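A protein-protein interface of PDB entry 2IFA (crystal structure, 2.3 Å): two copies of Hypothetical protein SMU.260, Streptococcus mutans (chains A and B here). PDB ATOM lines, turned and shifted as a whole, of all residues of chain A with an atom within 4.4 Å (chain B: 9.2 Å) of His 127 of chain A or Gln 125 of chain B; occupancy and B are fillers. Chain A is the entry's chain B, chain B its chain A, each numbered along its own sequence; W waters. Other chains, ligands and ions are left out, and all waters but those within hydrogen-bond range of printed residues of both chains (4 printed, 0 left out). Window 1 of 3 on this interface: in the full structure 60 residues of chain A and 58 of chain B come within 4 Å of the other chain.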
ATOM      1  N   LEU A  98     -25.416 -11.384  19.273  1.00  0.00           N
ATOM      2  CA  LEU A  98     -25.055 -12.025  20.538  1.00  0.00           C
ATOM      3  C   LEU A  98     -23.595 -11.787  20.859  1.00  0.00           C
ATOM      4  O   LEU A  98     -22.724 -12.031  20.028  1.00  0.00           O
ATOM      5  CB  LEU A  98     -25.302 -13.540  20.473  1.00  0.00           C
ATOM      6  CG  LEU A  98     -26.733 -13.991  20.206  1.00  0.00           C
ATOM      7  CD1 LEU A  98     -26.822 -15.504  20.215  1.00  0.00           C
ATOM      8  CD2 LEU A  98     -27.631 -13.397  21.274  1.00  0.00           C
ATOM      9  N   GLU A 100     -20.413 -11.944  24.169  1.00  0.00           N
ATOM     10  CA  GLU A 100     -20.003 -12.579  25.412  1.00  0.00           C
ATOM     11  C   GLU A 100     -19.140 -11.571  26.157  1.00  0.00           C
ATOM     12  O   GLU A 100     -18.156 -11.083  25.623  1.00  0.00           O
ATOM     13  CB  GLU A 100     -19.217 -13.871  25.134  1.00  0.00           C
ATOM     14  CG  GLU A 100     -20.105 -15.049  24.749  1.00  0.00           C
ATOM     15  CD  GLU A 100     -20.972 -15.527  25.906  1.00  0.00           C
ATOM     16  OE1 GLU A 100     -20.414 -15.858  26.976  1.00  0.00           O
ATOM     17  OE2 GLU A 100     -22.209 -15.577  25.748  1.00  0.00           O
ATOM     18  N   SER A 123     -17.667 -20.116  28.233  1.00  0.00           N
ATOM     19  CA  SER A 123     -18.288 -18.917  27.687  1.00  0.00           C
ATOM     20  C   SER A 123     -18.850 -19.238  26.299  1.00  0.00           C
ATOM     21  O   SER A 123     -20.005 -18.931  26.007  1.00  0.00           O
ATOM     22  CB  SER A 123     -17.285 -17.779  27.581  1.00  0.00           C
ATOM     23  OG  SER A 123     -17.846 -16.719  26.834  1.00  0.00           O
ATOM     24  N   GLU A 124     -18.036 -19.853  25.443  1.00  0.00           N
ATOM     25  CA  GLU A 124     -18.492 -20.245  24.102  1.00  0.00           C
ATOM     26  C   GLU A 124     -19.730 -21.160  24.279  1.00  0.00           C
ATOM     27  O   GLU A 124     -20.737 -21.003  23.586  1.00  0.00           O
ATOM     28  CB  GLU A 124     -17.396 -21.023  23.328  1.00  0.00           C
ATOM     29  CG  GLU A 124     -16.072 -20.276  23.020  1.00  0.00           C
ATOM     30  CD  GLU A 124     -16.264 -19.037  22.162  1.00  0.00           C
ATOM     31  OE1 GLU A 124     -17.207 -19.028  21.347  1.00  0.00           O
ATOM     32  OE2 GLU A 124     -15.467 -18.081  22.293  1.00  0.00           O
ATOM     33  N   GLN A 125     -19.647 -22.123  25.193  1.00  0.00           N
ATOM     34  CA  GLN A 125     -20.779 -23.030  25.416  1.00  0.00           C
ATOM     35  C   GLN A 125     -22.020 -22.249  25.873  1.00  0.00           C
ATOM     36  O   GLN A 125     -23.130 -22.536  25.419  1.00  0.00           O
ATOM     37  CB  GLN A 125     -20.401 -24.121  26.442  1.00  0.00           C
ATOM     38  CG  GLN A 125     -19.215 -24.990  25.992  1.00  0.00           C
ATOM     39  CD  GLN A 125     -18.649 -25.831  27.128  1.00  0.00           C
ATOM     40  OE1 GLN A 125     -17.673 -26.584  26.957  1.00  0.00           O
ATOM     41  NE2 GLN A 125     -19.252 -25.709  28.289  1.00  0.00           N
ATOM     42  N   ALA A 126     -21.822 -21.245  26.728  1.00  0.00           N
ATOM     43  CA  ALA A 126     -22.943 -20.428  27.209  1.00  0.00           C
ATOM     44  C   ALA A 126     -23.564 -19.676  26.042  1.00  0.00           C
ATOM     45  O   ALA A 126     -24.790 -19.535  25.977  1.00  0.00           O
ATOM     46  CB  ALA A 126     -22.475 -19.456  28.275  1.00  0.00           C
ATOM     47  N   HIS A 127     -22.727 -19.220  25.109  1.00  0.00           N
ATOM     48  CA  HIS A 127     -23.212 -18.511  23.929  1.00  0.00           C
ATOM     49  C   HIS A 127     -24.079 -19.416  23.070  1.00  0.00           C
ATOM     50  O   HIS A 127     -25.128 -19.002  22.563  1.00  0.00           O
ATOM     51  CB  HIS A 127     -22.049 -17.987  23.069  1.00  0.00           C
ATOM     52  CG  HIS A 127     -22.478 -17.556  21.699  1.00  0.00           C
ATOM     53  ND1 HIS A 127     -22.481 -18.416  20.617  1.00  0.00           N
ATOM     54  CD2 HIS A 127     -23.039 -16.405  21.263  1.00  0.00           C
ATOM     55  CE1 HIS A 127     -23.027 -17.816  19.575  1.00  0.00           C
ATOM     56  NE2 HIS A 127     -23.376 -16.595  19.941  1.00  0.00           N
ATOM     57  N   GLY A 128     -23.625 -20.655  22.893  1.00  0.00           N
ATOM     58  CA  GLY A 128     -24.376 -21.621  22.105  1.00  0.00           C
ATOM     59  C   GLY A 128     -25.734 -21.874  22.726  1.00  0.00           C
ATOM     60  O   GLY A 128     -26.749 -21.984  22.034  1.00  0.00           O
ATOM     61  N   ILE A 129     -25.753 -21.958  24.049  1.00  0.00           N
ATOM     62  CA  ILE A 129     -26.971 -22.183  24.818  1.00  0.00           C
ATOM     63  C   ILE A 129     -27.977 -21.046  24.663  1.00  0.00           C
ATOM     64  O   ILE A 129     -29.190 -21.278  24.593  1.00  0.00           O
ATOM     65  CB  ILE A 129     -26.622 -22.356  26.314  1.00  0.00           C
ATOM     66  CG1 ILE A 129     -25.813 -23.647  26.491  1.00  0.00           C
ATOM     67  CG2 ILE A 129     -27.901 -22.324  27.169  1.00  0.00           C
ATOM     68  CD1 ILE A 129     -25.434 -23.964  27.920  1.00  0.00           C
ATOM     69  N   ALA A 130     -27.477 -19.813  24.631  1.00  0.00           N
ATOM     70  CA  ALA A 130     -28.336 -18.651  24.484  1.00  0.00           C
ATOM     71  C   ALA A 130     -28.877 -18.673  23.055  1.00  0.00           C
ATOM     72  O   ALA A 130     -30.048 -18.389  22.819  1.00  0.00           O
ATOM     73  CB  ALA A 130     -27.543 -17.361  24.756  1.00  0.00           C
ATOM     74  N   LEU A 131     -28.017 -19.044  22.113  1.00  0.00           N
ATOM     75  CA  LEU A 131     -28.411 -19.132  20.710  1.00  0.00           C
ATOM     76  C   LEU A 131     -29.537 -20.155  20.528  1.00  0.00           C
ATOM     77  O   LEU A 131     -30.581 -19.846  19.958  1.00  0.00           O
ATOM     78  CB  LEU A 131     -27.210 -19.521  19.842  1.00  0.00           C
ATOM     79  CG  LEU A 131     -27.477 -19.846  18.365  1.00  0.00           C
ATOM     80  CD1 LEU A 131     -27.956 -18.599  17.649  1.00  0.00           C
ATOM     81  CD2 LEU A 131     -26.202 -20.377  17.714  1.00  0.00           C
ATOM     82  N   ARG A 171     -20.246 -12.617  18.869  1.00  0.00           N
ATOM     83  CA  ARG A 171     -20.115 -14.030  18.548  1.00  0.00           C
ATOM     84  C   ARG A 171     -21.038 -14.479  17.429  1.00  0.00           C
ATOM     85  O   ARG A 171     -20.780 -15.487  16.770  1.00  0.00           O
ATOM     86  CB  ARG A 171     -20.393 -14.876  19.799  1.00  0.00           C
ATOM     87  CG  ARG A 171     -19.626 -14.460  21.043  1.00  0.00           C
ATOM     88  CD  ARG A 171     -18.137 -14.336  20.762  1.00  0.00           C
ATOM     89  NE  ARG A 171     -17.561 -15.610  20.346  1.00  0.00           N
ATOM     90  CZ  ARG A 171     -16.646 -15.749  19.393  1.00  0.00           C
ATOM     91  NH1 ARG A 171     -16.184 -16.954  19.093  1.00  0.00           N
ATOM     92  NH2 ARG A 171     -16.212 -14.683  18.723  1.00  0.00           N
ATOM     93  N   ALA A 172     -22.115 -13.736  17.204  1.00  0.00           N
ATOM     94  CA  ALA A 172     -23.054 -14.110  16.162  1.00  0.00           C
ATOM     95  C   ALA A 172     -24.090 -13.042  15.843  1.00  0.00           C
ATOM     96  O   ALA A 172     -24.440 -12.221  16.674  1.00  0.00           O
ATOM     97  CB  ALA A 172     -23.763 -15.408  16.540  1.00  0.00           C
ATOM     98  N   ALA B  39     -29.784 -31.387  18.066  1.00  0.00           N
ATOM     99  CA  ALA B  39     -29.076 -30.186  18.459  1.00  0.00           C
ATOM    100  C   ALA B  39     -28.156 -29.827  17.270  1.00  0.00           C
ATOM    101  O   ALA B  39     -27.330 -30.639  16.856  1.00  0.00           O
ATOM    102  CB  ALA B  39     -28.278 -30.463  19.720  1.00  0.00           C
ATOM    103  N   PRO B  40     -28.316 -28.614  16.695  1.00  0.00           N
ATOM    104  CA  PRO B  40     -27.544 -28.106  15.551  1.00  0.00           C
ATOM    105  C   PRO B  40     -26.043 -27.997  15.804  1.00  0.00           C
ATOM    106  O   PRO B  40     -25.609 -27.891  16.947  1.00  0.00           O
ATOM    107  CB  PRO B  40     -28.181 -26.737  15.286  1.00  0.00           C
ATOM    108  CG  PRO B  40     -28.544 -26.289  16.644  1.00  0.00           C
ATOM    109  CD  PRO B  40     -29.140 -27.537  17.271  1.00  0.00           C
ATOM    110  N   SER B  41     -25.268 -28.025  14.720  1.00  0.00           N
ATOM    111  CA  SER B  41     -23.808 -27.916  14.774  1.00  0.00           C
ATOM    112  C   SER B  41     -23.332 -27.203  13.500  1.00  0.00           C
ATOM    113  O   SER B  41     -23.933 -27.368  12.437  1.00  0.00           O
ATOM    114  CB  SER B  41     -23.156 -29.309  14.878  1.00  0.00           C
ATOM    115  OG  SER B  41     -23.400 -30.109  13.730  1.00  0.00           O
ATOM    116  N   ALA B  42     -22.266 -26.410  13.619  1.00  0.00           N
ATOM    117  CA  ALA B  42     -21.697 -25.681  12.485  1.00  0.00           C
ATOM    118  C   ALA B  42     -21.516 -26.610  11.290  1.00  0.00           C
ATOM    119  O   ALA B  42     -20.948 -27.690  11.418  1.00  0.00           O
ATOM    120  CB  ALA B  42     -20.353 -25.074  12.875  1.00  0.00           C
ATOM    121  N   THR B  47     -20.142 -32.889  15.604  1.00  0.00           N
ATOM    122  CA  THR B  47     -18.950 -33.292  16.342  1.00  0.00           C
ATOM    123  C   THR B  47     -19.272 -33.819  17.736  1.00  0.00           C
ATOM    124  O   THR B  47     -18.388 -34.199  18.493  1.00  0.00           O
ATOM    125  CB  THR B  47     -18.025 -32.117  16.474  1.00  0.00           C
ATOM    126  OG1 THR B  47     -18.726 -31.042  17.108  1.00  0.00           O
ATOM    127  CG2 THR B  47     -17.562 -31.693  15.102  1.00  0.00           C
ATOM    128  N   SER B  48     -20.557 -33.829  18.043  1.00  0.00           N
ATOM    129  CA  SER B  48     -21.080 -34.277  19.317  1.00  0.00           C
ATOM    130  C   SER B  48     -21.032 -35.817  19.507  1.00  0.00           C
ATOM    131  O   SER B  48     -21.564 -36.556  18.689  1.00  0.00           O
ATOM    132  CB  SER B  48     -22.531 -33.805  19.408  1.00  0.00           C
ATOM    133  OG  SER B  48     -23.140 -34.379  20.532  1.00  0.00           O
ATOM    134  N   GLU B 100     -16.492 -34.148  22.184  1.00  0.00           N
ATOM    135  CA  GLU B 100     -16.464 -33.434  20.907  1.00  0.00           C
ATOM    136  C   GLU B 100     -15.385 -34.139  20.086  1.00  0.00           C
ATOM    137  O   GLU B 100     -14.245 -34.250  20.528  1.00  0.00           O
ATOM    138  CB  GLU B 100     -16.112 -31.957  21.100  1.00  0.00           C
ATOM    139  CG  GLU B 100     -17.261 -31.081  21.556  1.00  0.00           C
ATOM    140  CD  GLU B 100     -18.363 -30.949  20.504  1.00  0.00           C
ATOM    141  OE1 GLU B 100     -18.051 -30.509  19.366  1.00  0.00           O
ATOM    142  OE2 GLU B 100     -19.529 -31.284  20.822  1.00  0.00           O
ATOM    143  N   GLU B 117      -9.847 -20.826  12.437  1.00  0.00           N
ATOM    144  CA  GLU B 117      -9.964 -20.224  13.764  1.00  0.00           C
ATOM    145  C   GLU B 117     -11.314 -20.419  14.456  1.00  0.00           C
ATOM    146  O   GLU B 117     -11.380 -20.479  15.683  1.00  0.00           O
ATOM    147  CB  GLU B 117      -9.679 -18.718  13.668  1.00  0.00           C
ATOM    148  CG  GLU B 117      -8.313 -18.353  13.092  1.00  0.00           C
ATOM    149  CD  GLU B 117      -7.231 -18.241  14.155  1.00  0.00           C
ATOM    150  OE1 GLU B 117      -7.449 -17.510  15.147  1.00  0.00           O
ATOM    151  OE2 GLU B 117      -6.164 -18.878  13.994  1.00  0.00           O
ATOM    152  N   ASN B 118     -12.387 -20.510  13.677  1.00  0.00           N
ATOM    153  CA  ASN B 118     -13.724 -20.657  14.250  1.00  0.00           C
ATOM    154  C   ASN B 118     -14.172 -22.082  14.591  1.00  0.00           C
ATOM    155  O   ASN B 118     -15.073 -22.263  15.407  1.00  0.00           O
ATOM    156  CB  ASN B 118     -14.769 -20.036  13.313  1.00  0.00           C
ATOM    157  CG  ASN B 118     -14.505 -18.576  13.028  1.00  0.00           C
ATOM    158  OD1 ASN B 118     -14.273 -17.784  13.940  1.00  0.00           O
ATOM    159  ND2 ASN B 118     -14.542 -18.209  11.750  1.00  0.00           N
ATOM    160  N   PHE B 119     -13.556 -23.087  13.981  1.00  0.00           N
ATOM    161  CA  PHE B 119     -13.982 -24.460  14.241  1.00  0.00           C
ATOM    162  C   PHE B 119     -13.924 -24.876  15.702  1.00  0.00           C
ATOM    163  O   PHE B 119     -14.838 -25.523  16.209  1.00  0.00           O
ATOM    164  CB  PHE B 119     -13.181 -25.425  13.368  1.00  0.00           C
ATOM    165  CG  PHE B 119     -13.458 -25.262  11.897  1.00  0.00           C
ATOM    166  CD1 PHE B 119     -14.740 -25.464  11.390  1.00  0.00           C
ATOM    167  CD2 PHE B 119     -12.446 -24.883  11.025  1.00  0.00           C
ATOM    168  CE1 PHE B 119     -15.008 -25.291  10.029  1.00  0.00           C
ATOM    169  CE2 PHE B 119     -12.706 -24.707   9.660  1.00  0.00           C
ATOM    170  CZ  PHE B 119     -13.985 -24.912   9.163  1.00  0.00           C
ATOM    171  N   GLN B 120     -12.863 -24.479  16.391  1.00  0.00           N
ATOM    172  CA  GLN B 120     -12.722 -24.829  17.792  1.00  0.00           C
ATOM    173  C   GLN B 120     -13.846 -24.191  18.620  1.00  0.00           C
ATOM    174  O   GLN B 120     -14.537 -24.886  19.354  1.00  0.00           O
ATOM    175  CB  GLN B 120     -11.341 -24.406  18.312  1.00  0.00           C
ATOM    176  CG  GLN B 120     -10.893 -25.183  19.507  1.00  0.00           C
ATOM    177  CD  GLN B 120     -10.960 -26.696  19.261  1.00  0.00           C
ATOM    178  OE1 GLN B 120     -10.157 -27.253  18.521  1.00  0.00           O
ATOM    179  NE2 GLN B 120     -11.918 -27.351  19.878  1.00  0.00           N
ATOM    180  N   PRO B 121     -14.031 -22.862  18.516  1.00  0.00           N
ATOM    181  CA  PRO B 121     -15.092 -22.179  19.267  1.00  0.00           C
ATOM    182  C   PRO B 121     -16.491 -22.665  18.876  1.00  0.00           C
ATOM    183  O   PRO B 121     -17.357 -22.864  19.738  1.00  0.00           O
ATOM    184  CB  PRO B 121     -14.872 -20.710  18.920  1.00  0.00           C
ATOM    185  CG  PRO B 121     -13.378 -20.634  18.742  1.00  0.00           C
ATOM    186  CD  PRO B 121     -13.083 -21.885  17.941  1.00  0.00           C
ATOM    187  N   TRP B 122     -16.719 -22.856  17.580  1.00  0.00           N
ATOM    188  CA  TRP B 122     -18.012 -23.345  17.128  1.00  0.00           C
ATOM    189  C   TRP B 122     -18.262 -24.762  17.647  1.00  0.00           C
ATOM    190  O   TRP B 122     -19.415 -25.180  17.784  1.00  0.00           O
ATOM    191  CB  TRP B 122     -18.113 -23.327  15.603  1.00  0.00           C
ATOM    192  CG  TRP B 122     -18.263 -21.944  15.007  1.00  0.00           C
ATOM    193  CD1 TRP B 122     -18.737 -20.834  15.630  1.00  0.00           C
ATOM    194  CD2 TRP B 122     -17.977 -21.559  13.662  1.00  0.00           C
ATOM    195  NE1 TRP B 122     -18.767 -19.771  14.761  1.00  0.00           N
ATOM    196  CE2 TRP B 122     -18.304 -20.189  13.544  1.00  0.00           C
ATOM    197  CE3 TRP B 122     -17.475 -22.238  12.543  1.00  0.00           C
ATOM    198  CZ2 TRP B 122     -18.147 -19.477  12.349  1.00  0.00           C
ATOM    199  CZ3 TRP B 122     -17.315 -21.530  11.343  1.00  0.00           C
ATOM    200  CH2 TRP B 122     -17.652 -20.161  11.258  1.00  0.00           C
ATOM    201  N   SER B 123     -17.191 -25.507  17.924  1.00  0.00           N
ATOM    202  CA  SER B 123     -17.350 -26.859  18.447  1.00  0.00           C
ATOM    203  C   SER B 123     -17.795 -26.773  19.903  1.00  0.00           C
ATOM    204  O   SER B 123     -18.688 -27.520  20.321  1.00  0.00           O
ATOM    205  CB  SER B 123     -16.047 -27.662  18.346  1.00  0.00           C
ATOM    206  OG  SER B 123     -16.192 -28.964  18.894  1.00  0.00           O
ATOM    207  N   GLU B 124     -17.200 -25.854  20.667  1.00  0.00           N
ATOM    208  CA  GLU B 124     -17.561 -25.668  22.073  1.00  0.00           C
ATOM    209  C   GLU B 124     -19.020 -25.190  22.160  1.00  0.00           C
ATOM    210  O   GLU B 124     -19.778 -25.593  23.051  1.00  0.00           O
ATOM    211  CB  GLU B 124     -16.638 -24.637  22.729  1.00  0.00           C
ATOM    212  CG  GLU B 124     -15.176 -25.051  22.904  1.00  0.00           C
ATOM    213  CD  GLU B 124     -14.998 -26.227  23.864  1.00  0.00           C
ATOM    214  OE1 GLU B 124     -15.945 -26.502  24.628  1.00  0.00           O
ATOM    215  OE2 GLU B 124     -13.915 -26.867  23.868  1.00  0.00           O
ATOM    216  N   GLN B 125     -19.411 -24.339  21.218  1.00  0.00           N
ATOM    217  CA  GLN B 125     -20.767 -23.821  21.174  1.00  0.00           C
ATOM    218  C   GLN B 125     -21.742 -24.978  20.936  1.00  0.00           C
ATOM    219  O   GLN B 125     -22.757 -25.085  21.624  1.00  0.00           O
ATOM    220  CB  GLN B 125     -20.884 -22.747  20.077  1.00  0.00           C
ATOM    221  CG  GLN B 125     -20.077 -21.496  20.418  1.00  0.00           C
ATOM    222  CD  GLN B 125     -19.967 -20.477  19.270  1.00  0.00           C
ATOM    223  OE1 GLN B 125     -19.165 -19.561  19.336  1.00  0.00           O
ATOM    224  NE2 GLN B 125     -20.766 -20.640  18.237  1.00  0.00           N
ATOM    225  N   ALA B 126     -21.417 -25.857  19.994  1.00  0.00           N
ATOM    226  CA  ALA B 126     -22.264 -27.006  19.672  1.00  0.00           C
ATOM    227  C   ALA B 126     -22.411 -27.957  20.868  1.00  0.00           C
ATOM    228  O   ALA B 126     -23.433 -28.616  21.024  1.00  0.00           O
ATOM    229  CB  ALA B 126     -21.683 -27.767  18.474  1.00  0.00           C
ATOM    230  N   HIS B 127     -21.380 -28.026  21.700  1.00  0.00           N
ATOM    231  CA  HIS B 127     -21.417 -28.900  22.873  1.00  0.00           C
ATOM    232  C   HIS B 127     -22.443 -28.338  23.839  1.00  0.00           C
ATOM    233  O   HIS B 127     -23.283 -29.066  24.362  1.00  0.00           O
ATOM    234  CB  HIS B 127     -20.041 -28.949  23.558  1.00  0.00           C
ATOM    235  CG  HIS B 127     -20.102 -29.357  24.994  1.00  0.00           C
ATOM    236  ND1 HIS B 127     -20.211 -30.671  25.395  1.00  0.00           N
ATOM    237  CD2 HIS B 127     -20.145 -28.615  26.125  1.00  0.00           C
ATOM    238  CE1 HIS B 127     -20.319 -30.717  26.711  1.00  0.00           C
ATOM    239  NE2 HIS B 127     -20.282 -29.482  27.179  1.00  0.00           N
ATOM    240  N   GLY B 128     -22.356 -27.026  24.058  1.00  0.00           N
ATOM    241  CA  GLY B 128     -23.268 -26.337  24.950  1.00  0.00           C
ATOM    242  C   GLY B 128     -24.697 -26.561  24.512  1.00  0.00           C
ATOM    243  O   GLY B 128     -25.564 -26.813  25.339  1.00  0.00           O
ATOM    244  N   ILE B 129     -24.931 -26.450  23.209  1.00  0.00           N
ATOM    245  CA  ILE B 129     -26.255 -26.649  22.619  1.00  0.00           C
ATOM    246  C   ILE B 129     -26.742 -28.077  22.870  1.00  0.00           C
ATOM    247  O   ILE B 129     -27.927 -28.302  23.130  1.00  0.00           O
ATOM    248  CB  ILE B 129     -26.219 -26.405  21.085  1.00  0.00           C
ATOM    249  CG1 ILE B 129     -25.930 -24.937  20.793  1.00  0.00           C
ATOM    250  CG2 ILE B 129     -27.541 -26.819  20.455  1.00  0.00           C
ATOM    251  CD1 ILE B 129     -25.754 -24.652  19.314  1.00  0.00           C
ATOM    252  N   ALA B 130     -25.829 -29.039  22.774  1.00  0.00           N
ATOM    253  CA  ALA B 130     -26.199 -30.426  23.009  1.00  0.00           C
ATOM    254  C   ALA B 130     -26.548 -30.586  24.483  1.00  0.00           C
ATOM    255  O   ALA B 130     -27.535 -31.254  24.827  1.00  0.00           O
ATOM    256  CB  ALA B 130     -25.057 -31.370  22.615  1.00  0.00           C
ATOM    257  N   LEU B 131     -25.752 -29.959  25.349  1.00  0.00           N
ATOM    258  CA  LEU B 131     -25.985 -30.013  26.792  1.00  0.00           C
ATOM    259  C   LEU B 131     -27.365 -29.465  27.161  1.00  0.00           C
ATOM    260  O   LEU B 131     -28.104 -30.074  27.922  1.00  0.00           O
ATOM    261  CB  LEU B 131     -24.919 -29.206  27.536  1.00  0.00           C
ATOM    262  CG  LEU B 131     -25.086 -28.989  29.047  1.00  0.00           C
ATOM    263  CD1 LEU B 131     -24.702 -30.257  29.808  1.00  0.00           C
ATOM    264  CD2 LEU B 131     -24.198 -27.829  29.485  1.00  0.00           C
ATOM    265  N   TYR B 132     -27.705 -28.310  26.607  1.00  0.00           N
ATOM    266  CA  TYR B 132     -28.981 -27.677  26.898  1.00  0.00           C
ATOM    267  C   TYR B 132     -30.134 -28.496  26.338  1.00  0.00           C
ATOM    268  O   TYR B 132     -31.213 -28.551  26.925  1.00  0.00           O
ATOM    269  CB  TYR B 132     -28.992 -26.254  26.309  1.00  0.00           C
ATOM    270  CG  TYR B 132     -30.080 -25.353  26.864  1.00  0.00           C
ATOM    271  CD1 TYR B 132     -30.331 -25.297  28.234  1.00  0.00           C
ATOM    272  CD2 TYR B 132     -30.852 -24.564  26.018  1.00  0.00           C
ATOM    273  CE1 TYR B 132     -31.335 -24.486  28.750  1.00  0.00           C
ATOM    274  CE2 TYR B 132     -31.851 -23.745  26.514  1.00  0.00           C
ATOM    275  CZ  TYR B 132     -32.098 -23.713  27.888  1.00  0.00           C
ATOM    276  OH  TYR B 132     -33.144 -22.956  28.394  1.00  0.00           O
ATOM    277  N   ALA B 133     -29.900 -29.131  25.194  1.00  0.00           N
ATOM    278  CA  ALA B 133     -30.913 -29.948  24.542  1.00  0.00           C
ATOM    279  C   ALA B 133     -31.318 -31.121  25.436  1.00  0.00           C
ATOM    280  O   ALA B 133     -32.496 -31.449  25.539  1.00  0.00           O
ATOM    281  CB  ALA B 133     -30.381 -30.466  23.219  1.00  0.00           C
ATOM    282  N   ARG B 171     -15.947 -33.216  27.394  1.00  0.00           N
ATOM    283  CA  ARG B 171     -16.226 -31.843  27.789  1.00  0.00           C
ATOM    284  C   ARG B 171     -17.146 -31.724  28.987  1.00  0.00           C
ATOM    285  O   ARG B 171     -17.227 -30.667  29.586  1.00  0.00           O
ATOM    286  CB  ARG B 171     -16.857 -31.046  26.642  1.00  0.00           C
ATOM    287  CG  ARG B 171     -16.228 -31.243  25.275  1.00  0.00           C
ATOM    288  CD  ARG B 171     -14.741 -30.908  25.270  1.00  0.00           C
ATOM    289  NE  ARG B 171     -14.432 -29.505  25.532  1.00  0.00           N
ATOM    290  CZ  ARG B 171     -13.452 -29.124  26.347  1.00  0.00           C
ATOM    291  NH1 ARG B 171     -13.181 -27.843  26.539  1.00  0.00           N
ATOM    292  NH2 ARG B 171     -12.752 -30.036  27.001  1.00  0.00           N
HETATM  293  O   HOH W   1     -18.917 -17.583  17.115  1.00  0.00           O
HETATM  294  O   HOH W   2     -16.189 -28.013  29.211  1.00  0.00           O
HETATM  295  O   HOH W   3     -14.563 -17.026  16.671  1.00  0.00           O
HETATM  296  O   HOH W   4     -19.863 -28.291  29.538  1.00  0.00           O
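The side-chain carboxylate (OE1) of Glu 124 of chain B lies close to the side-chain amide oxygen (OE1) of Gln 125 of chain A (2.9 Å). OE1 of Gln 125 of chain B sits close to OE1 of Glu 124 of chain A, at 2.9 Å.
Hydrophobic or aromatic side chains of chain A that line the printed part of chain B: His 127 and Ile 129. Printed residues of chain B that touch a printed residue of chain A: Pro 121, Glu 124, Gln 125, His 127, Gly 128, Ile 129 and Tyr 132. Hydrophobic or aromatic side chains of chain B within 4 Å of the printed part of chain A: Pro 121, His 127, Ile 129 and Tyr 132. Among the printed residues, no Asp or Glu carboxylate lies within 4 Å of a Lys or Arg side-chain nitrogen of the other chain.
Glu 124 of chain A touches just these residues of chain B: Pro 121, Glu 124 and Gln 125. His 127 of chain A touches just one residue of chain B: Gln 125. Of chain B, only Gln 125 and Ile 129 come within 4 Å of Gly 128 of chain A. Of the printed residues of chain B, Arg 171 of chain A touches Pro 121 (3.98 Å) and Gln 125 (3.97 Å). Glu 117 of chain B touches none of the printed residues of chain A. Of the printed residues of chain A, His 127 of chain B touches Gln 125. Of the printed residues of chain A, Gly 128 of chain B touches Gln 125 (3.8 Å) and Ile 129 (3.4 Å). Of the printed residues of chain A, Tyr 132 of chain B touches Ile 129 (3.7 Å). The nearest residue of chain A that does not touch Gln 125 of chain B is Gln 125 of chain A (4.3 Å).
Water W4 bridges NE2 of His 127 of chain B (2.7 Å) and NE2 of Gln 125 of chain A (2.9 Å). Water W1 lies within hydrogen-bond range of the backbone carbonyl oxygen (O) of Arg 171 of chain A, the side-chain amide oxygen (OE1) of Gln 125 of chain B and the indole nitrogen (NE1) of Trp 122 of chain B. Water W3 lies within hydrogen-bond range of the side-chain amide oxygen (OD1) of Asn 118 of chain B (2.8 Å) and the guanidinium group (NH1) of Arg 171 of chain A (2.9 Å). Water W2 lies within hydrogen-bond range of O of Arg 171 of chain B (2.9 Å) and OE1 of Gln 125 of chain A (3.1 Å).
The guanidinium group of Arg 171 of chain B is in salt-bridge range of the side-chain carboxylate of Glu 124 of chain B (2.9 Å). The backbone NH (N) of Arg 171 of chain A lies within hydrogen-bond range of the backbone carbonyl oxygen (O) of Leu 98 of chain A. OE1 of Glu 124 of chain A is in salt-bridge range of NH1 of Arg 171 of chain A, 3.2 Å away.
Pro 121 of chain B touches Glu 124 of chain A. Glu 124 of chain B touches Glu 124 of chain A (CB to CB, 3.7 Å). Gln 125 of chain A touches His 127 of chain B. Gln 125 of chain B touches His 127 of chain A (CD to ND1, 3.5 Å). O of Gln 125 of chain B touches CA of Gly 128 of chain A, at 3.9 Å. Gly 128 of chain A touches Ile 129 of chain B (O to CG1, 3.3 Å). Ile 129 of chain A touches Gly 128 of chain B. Ile 129 of chain A touches Tyr 132 of chain B (CG2 to CG, 3.7 Å). Pro 121 of chain B touches Arg 171 of chain A (CB to NH1, 3.98 Å). OE1 of Gln 125 of chain B touches NH1 of Arg 171 of chain A, 3.97 Å away.
Glu 124 of chain A touches Gln 125 of chain B, and with the chains exchanged Gln 125 of chain A touches Glu 124 of chain B. Gln 125 of chain A touches His 127 of chain B, and with the chains exchanged His 127 of chain A touches Gln 125 of chain B. Gln 125 of chain A touches Gly 128 of chain B, and with the chains exchanged Gly 128 of chain A touches Gln 125 of chain B. Arg 171 of chain A touches Gln 125 of chain B, but with the chains exchanged Gln 125 of chain A does not touch Arg 171 of chain B (4.5 Å). Positions printed for both chains: 100, 123, 124, 125, 126, 127, 128, 129, 130, 131 and 171. Of the 13 pairs that touch across the chains among the printed residues, 9 have their exchanged pair printed and touching as well.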
